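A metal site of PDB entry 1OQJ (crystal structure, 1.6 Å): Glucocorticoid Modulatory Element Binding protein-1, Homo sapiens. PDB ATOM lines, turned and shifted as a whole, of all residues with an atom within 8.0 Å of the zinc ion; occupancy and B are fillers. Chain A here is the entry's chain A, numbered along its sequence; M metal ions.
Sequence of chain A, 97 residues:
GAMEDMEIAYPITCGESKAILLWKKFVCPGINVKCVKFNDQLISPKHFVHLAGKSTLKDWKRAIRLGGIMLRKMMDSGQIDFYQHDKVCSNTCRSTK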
ATOM      1  N   VAL A  27      -0.889 -25.406   7.938  1.00  0.00           N
ATOM      2  CA  VAL A  27      -2.021 -25.462   7.020  1.00  0.00           C
ATOM      3  C   VAL A  27      -3.268 -26.075   7.656  1.00  0.00           C
ATOM      4  O   VAL A  27      -3.181 -27.050   8.393  1.00  0.00           O
ATOM      5  CB  VAL A  27      -1.618 -26.275   5.767  1.00  0.00           C
ATOM      6  CG1 VAL A  27      -2.781 -26.359   4.789  1.00  0.00           C
ATOM      7  CG2 VAL A  27      -0.411 -25.622   5.105  1.00  0.00           C
ATOM      8  N   CYS A  28      -4.428 -25.489   7.362  1.00  0.00           N
ATOM      9  CA  CYS A  28      -5.683 -25.999   7.907  1.00  0.00           C
ATOM     10  C   CYS A  28      -5.844 -27.487   7.569  1.00  0.00           C
ATOM     11  O   CYS A  28      -5.556 -27.894   6.443  1.00  0.00           O
ATOM     12  CB  CYS A  28      -6.859 -25.219   7.323  1.00  0.00           C
ATOM     13  SG  CYS A  28      -8.475 -25.824   7.853  1.00  0.00           S
ATOM     14  N   PRO A  29      -6.370 -28.295   8.512  1.00  0.00           N
ATOM     15  CA  PRO A  29      -6.826 -27.959   9.864  1.00  0.00           C
ATOM     16  C   PRO A  29      -5.753 -28.009  10.946  1.00  0.00           C
ATOM     17  O   PRO A  29      -6.063 -28.035  12.146  1.00  0.00           O
ATOM     18  CB  PRO A  29      -7.930 -28.973  10.098  1.00  0.00           C
ATOM     19  CG  PRO A  29      -7.343 -30.193   9.480  1.00  0.00           C
ATOM     20  CD  PRO A  29      -6.719 -29.682   8.184  1.00  0.00           C
ATOM     21  N   GLY A  30      -4.492 -28.065  10.513  1.00  0.00           N
ATOM     22  CA  GLY A  30      -3.363 -28.078  11.424  1.00  0.00           C
ATOM     23  C   GLY A  30      -3.103 -29.226  12.376  1.00  0.00           C
ATOM     24  O   GLY A  30      -1.945 -29.610  12.572  1.00  0.00           O
ATOM     25  N   LYS A  61      -5.620 -26.101  20.076  1.00  0.00           N
ATOM     26  CA  LYS A  61      -5.542 -24.671  19.834  1.00  0.00           C
ATOM     27  C   LYS A  61      -5.525 -23.863  21.125  1.00  0.00           C
ATOM     28  O   LYS A  61      -5.062 -22.728  21.147  1.00  0.00           O
ATOM     29  CB  LYS A  61      -6.696 -24.191  18.962  1.00  0.00           C
ATOM     30  CG  LYS A  61      -6.785 -24.884  17.618  1.00  0.00           C
ATOM     31  CD  LYS A  61      -7.892 -24.293  16.758  1.00  0.00           C
ATOM     32  CE  LYS A  61      -8.230 -25.197  15.586  1.00  0.00           C
ATOM     33  NZ  LYS A  61      -8.830 -26.487  16.051  1.00  0.00           N
ATOM     34  N   MET A  75      -5.066 -17.039  16.077  1.00  0.00           N
ATOM     35  CA  MET A  75      -5.614 -17.503  14.815  1.00  0.00           C
ATOM     36  C   MET A  75      -6.888 -16.722  14.481  1.00  0.00           C
ATOM     37  O   MET A  75      -7.063 -16.251  13.349  1.00  0.00           O
ATOM     38  CB  MET A  75      -5.941 -18.995  14.885  1.00  0.00           C
ATOM     39  CG  MET A  75      -4.709 -19.890  15.027  1.00  0.00           C
ATOM     40  SD  MET A  75      -5.138 -21.574  15.498  1.00  0.00           S
ATOM     41  CE  MET A  75      -5.829 -22.183  13.984  1.00  0.00           C
ATOM     42  N   ASP A  81      -3.018 -17.038  11.634  1.00  0.00           N
ATOM     43  CA  ASP A  81      -3.976 -18.077  11.272  1.00  0.00           C
ATOM     44  C   ASP A  81      -3.276 -19.024  10.285  1.00  0.00           C
ATOM     45  O   ASP A  81      -2.132 -18.787   9.904  1.00  0.00           O
ATOM     46  CB  ASP A  81      -5.199 -17.430  10.616  1.00  0.00           C
ATOM     47  CG  ASP A  81      -6.386 -18.369  10.510  1.00  0.00           C
ATOM     48  OD1 ASP A  81      -6.380 -19.425  11.175  1.00  0.00           O
ATOM     49  OD2 ASP A  81      -7.327 -18.039   9.756  1.00  0.00           O
ATOM     50  N   PHE A  82      -3.952 -20.103   9.897  1.00  0.00           N
ATOM     51  CA  PHE A  82      -3.355 -21.043   8.961  1.00  0.00           C
ATOM     52  C   PHE A  82      -2.884 -20.335   7.696  1.00  0.00           C
ATOM     53  O   PHE A  82      -3.544 -19.393   7.222  1.00  0.00           O
ATOM     54  CB  PHE A  82      -4.381 -22.102   8.551  1.00  0.00           C
ATOM     55  CG  PHE A  82      -4.871 -22.946   9.683  1.00  0.00           C
ATOM     56  CD1 PHE A  82      -6.229 -22.987   9.999  1.00  0.00           C
ATOM     57  CD2 PHE A  82      -3.993 -23.745  10.402  1.00  0.00           C
ATOM     58  CE1 PHE A  82      -6.710 -23.819  11.022  1.00  0.00           C
ATOM     59  CE2 PHE A  82      -4.457 -24.579  11.422  1.00  0.00           C
ATOM     60  CZ  PHE A  82      -5.822 -24.619  11.731  1.00  0.00           C
ATOM     61  N   GLN A  84      -2.586 -19.257   4.112  1.00  0.00           N
ATOM     62  CA  GLN A  84      -3.538 -19.246   2.998  1.00  0.00           C
ATOM     63  C   GLN A  84      -4.906 -19.779   3.395  1.00  0.00           C
ATOM     64  O   GLN A  84      -5.605 -20.373   2.579  1.00  0.00           O
ATOM     65  CB  GLN A  84      -3.001 -20.089   1.833  1.00  0.00           C
ATOM     66  CG  GLN A  84      -1.663 -19.647   1.294  1.00  0.00           C
ATOM     67  CD  GLN A  84      -1.284 -20.407   0.031  1.00  0.00           C
ATOM     68  OE1 GLN A  84      -1.025 -21.612   0.069  1.00  0.00           O
ATOM     69  NE2 GLN A  84      -1.256 -19.705  -1.089  1.00  0.00           N
ATOM     70  N   HIS A  85      -5.317 -19.541   4.640  1.00  0.00           N
ATOM     71  CA  HIS A  85      -6.602 -20.056   5.098  1.00  0.00           C
ATOM     72  C   HIS A  85      -7.817 -19.621   4.283  1.00  0.00           C
ATOM     73  O   HIS A  85      -8.811 -20.355   4.225  1.00  0.00           O
ATOM     74  CB  HIS A  85      -6.827 -19.688   6.576  1.00  0.00           C
ATOM     75  CG  HIS A  85      -7.764 -20.622   7.276  1.00  0.00           C
ATOM     76  ND1 HIS A  85      -8.285 -20.358   8.524  1.00  0.00           N
ATOM     77  CD2 HIS A  85      -8.250 -21.834   6.915  1.00  0.00           C
ATOM     78  CE1 HIS A  85      -9.060 -21.359   8.896  1.00  0.00           C
ATOM     79  NE2 HIS A  85      -9.049 -22.274   7.939  1.00  0.00           N
ATOM     80  N   ASP A  86      -7.751 -18.452   3.663  1.00  0.00           N
ATOM     81  CA  ASP A  86      -8.878 -17.995   2.875  1.00  0.00           C
ATOM     82  C   ASP A  86      -9.100 -18.840   1.621  1.00  0.00           C
ATOM     83  O   ASP A  86     -10.172 -18.775   1.021  1.00  0.00           O
ATOM     84  CB  ASP A  86      -8.705 -16.520   2.481  1.00  0.00           C
ATOM     85  CG  ASP A  86      -7.452 -16.281   1.664  1.00  0.00           C
ATOM     86  OD1 ASP A  86      -7.317 -15.179   1.107  1.00  0.00           O
ATOM     87  OD2 ASP A  86      -6.600 -17.185   1.590  1.00  0.00           O
ATOM     88  N   VAL A  88      -7.312 -22.274   1.398  1.00  0.00           N
ATOM     89  CA  VAL A  88      -7.009 -23.651   1.773  1.00  0.00           C
ATOM     90  C   VAL A  88      -7.647 -23.959   3.114  1.00  0.00           C
ATOM     91  O   VAL A  88      -7.183 -23.497   4.158  1.00  0.00           O
ATOM     92  CB  VAL A  88      -5.488 -23.863   1.845  1.00  0.00           C
ATOM     93  CG1 VAL A  88      -5.170 -25.288   2.270  1.00  0.00           C
ATOM     94  CG2 VAL A  88      -4.860 -23.559   0.484  1.00  0.00           C
ATOM     95  N   CYS A  89      -8.724 -24.749   3.091  1.00  0.00           N
ATOM     96  CA  CYS A  89      -9.458 -25.091   4.310  1.00  0.00           C
ATOM     97  C   CYS A  89     -10.124 -26.454   4.190  1.00  0.00           C
ATOM     98  O   CYS A  89     -10.567 -26.850   3.120  1.00  0.00           O
ATOM     99  CB  CYS A  89     -10.513 -24.004   4.582  1.00  0.00           C
ATOM    100  SG  CYS A  89     -11.490 -24.199   6.095  1.00  0.00           S
ATOM    101  N   SER A  90     -10.207 -27.174   5.306  1.00  0.00           N
ATOM    102  CA  SER A  90     -10.823 -28.495   5.315  1.00  0.00           C
ATOM    103  C   SER A  90     -12.263 -28.435   5.791  1.00  0.00           C
ATOM    104  O   SER A  90     -12.995 -29.420   5.696  1.00  0.00           O
ATOM    105  CB  SER A  90     -10.064 -29.432   6.255  1.00  0.00           C
ATOM    106  OG  SER A  90     -10.214 -28.997   7.592  1.00  0.00           O
ATOM    107  N   ASN A  91     -12.657 -27.280   6.326  1.00  0.00           N
ATOM    108  CA  ASN A  91     -14.011 -27.085   6.835  1.00  0.00           C
ATOM    109  C   ASN A  91     -14.246 -27.884   8.115  1.00  0.00           C
ATOM    110  O   ASN A  91     -15.379 -28.143   8.496  1.00  0.00           O
ATOM    111  CB  ASN A  91     -15.035 -27.496   5.776  1.00  0.00           C
ATOM    112  CG  ASN A  91     -14.840 -26.775   4.454  1.00  0.00           C
ATOM    113  OD1 ASN A  91     -14.933 -25.554   4.389  1.00  0.00           O
ATOM    114  ND2 ASN A  91     -14.561 -27.530   3.399  1.00  0.00           N
ATOM    115  N   THR A  92     -13.158 -28.289   8.761  1.00  0.00           N
ATOM    116  CA  THR A  92     -13.245 -29.050  10.008  1.00  0.00           C
ATOM    117  C   THR A  92     -12.404 -28.375  11.081  1.00  0.00           C
ATOM    118  O   THR A  92     -12.258 -28.893  12.192  1.00  0.00           O
ATOM    119  CB  THR A  92     -12.738 -30.497   9.849  1.00  0.00           C
ATOM    120  OG1 THR A  92     -11.323 -30.483   9.557  1.00  0.00           O
ATOM    121  CG2 THR A  92     -13.473 -31.200   8.719  1.00  0.00           C
ATOM    122  N   CYS A  93     -11.851 -27.217  10.749  1.00  0.00           N
ATOM    123  CA  CYS A  93     -11.014 -26.477  11.675  1.00  0.00           C
ATOM    124  C   CYS A  93     -11.798 -25.855  12.818  1.00  0.00           C
ATOM    125  O   CYS A  93     -11.223 -25.483  13.847  1.00  0.00           O
ATOM    126  CB  CYS A  93     -10.241 -25.388  10.925  1.00  0.00           C
ATOM    127  SG  CYS A  93     -11.278 -24.289   9.923  1.00  0.00           S
ATOM    128  N   ARG A  94     -13.112 -25.765  12.654  1.00  0.00           N
ATOM    129  CA  ARG A  94     -13.979 -25.206  13.685  1.00  0.00           C
ATOM    130  C   ARG A  94     -14.703 -26.325  14.422  1.00  0.00           C
ATOM    131  O   ARG A  94     -15.951 -26.323  14.395  1.00  0.00           O
ATOM    132  CB  ARG A  94     -14.991 -24.250  13.042  1.00  0.00           C
HETATM  133 ZN    ZN M   1     -10.002 -24.140   7.940  1.00  0.00          ZN
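The zinc ion is bound by a ring nitrogen (NE2) of His 85 (2.1 Å), the side-chain sulfur (SG) of Cys 28 (2.3 Å), the side-chain sulfur (SG) of Cys 93 (2.4 Å) and the side-chain sulfur (SG) of Cys 89 (2.4 Å).
The zinc ion has four donor atoms within binding distance.
Four residues have an atom within 4 Å of the zinc ion: Cys 28, His 85, Cys 89 and Cys 93.
A ring nitrogen (ND1) of His 85 lies within hydrogen-bond range of the side-chain carboxylate (OD2) of Asp 81 (2.8 Å).
SG of Cys 28 sits close to N of Ser 90 (3.4 Å).
The backbone carbonyl oxygen (O) of Cys 93 sits at hydrogen-bond distance from the side-chain amino group (NZ) of Lys 61 (3.4 Å).
N of Asn 91 sits close to SG of Cys 89, at 3.3 Å.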
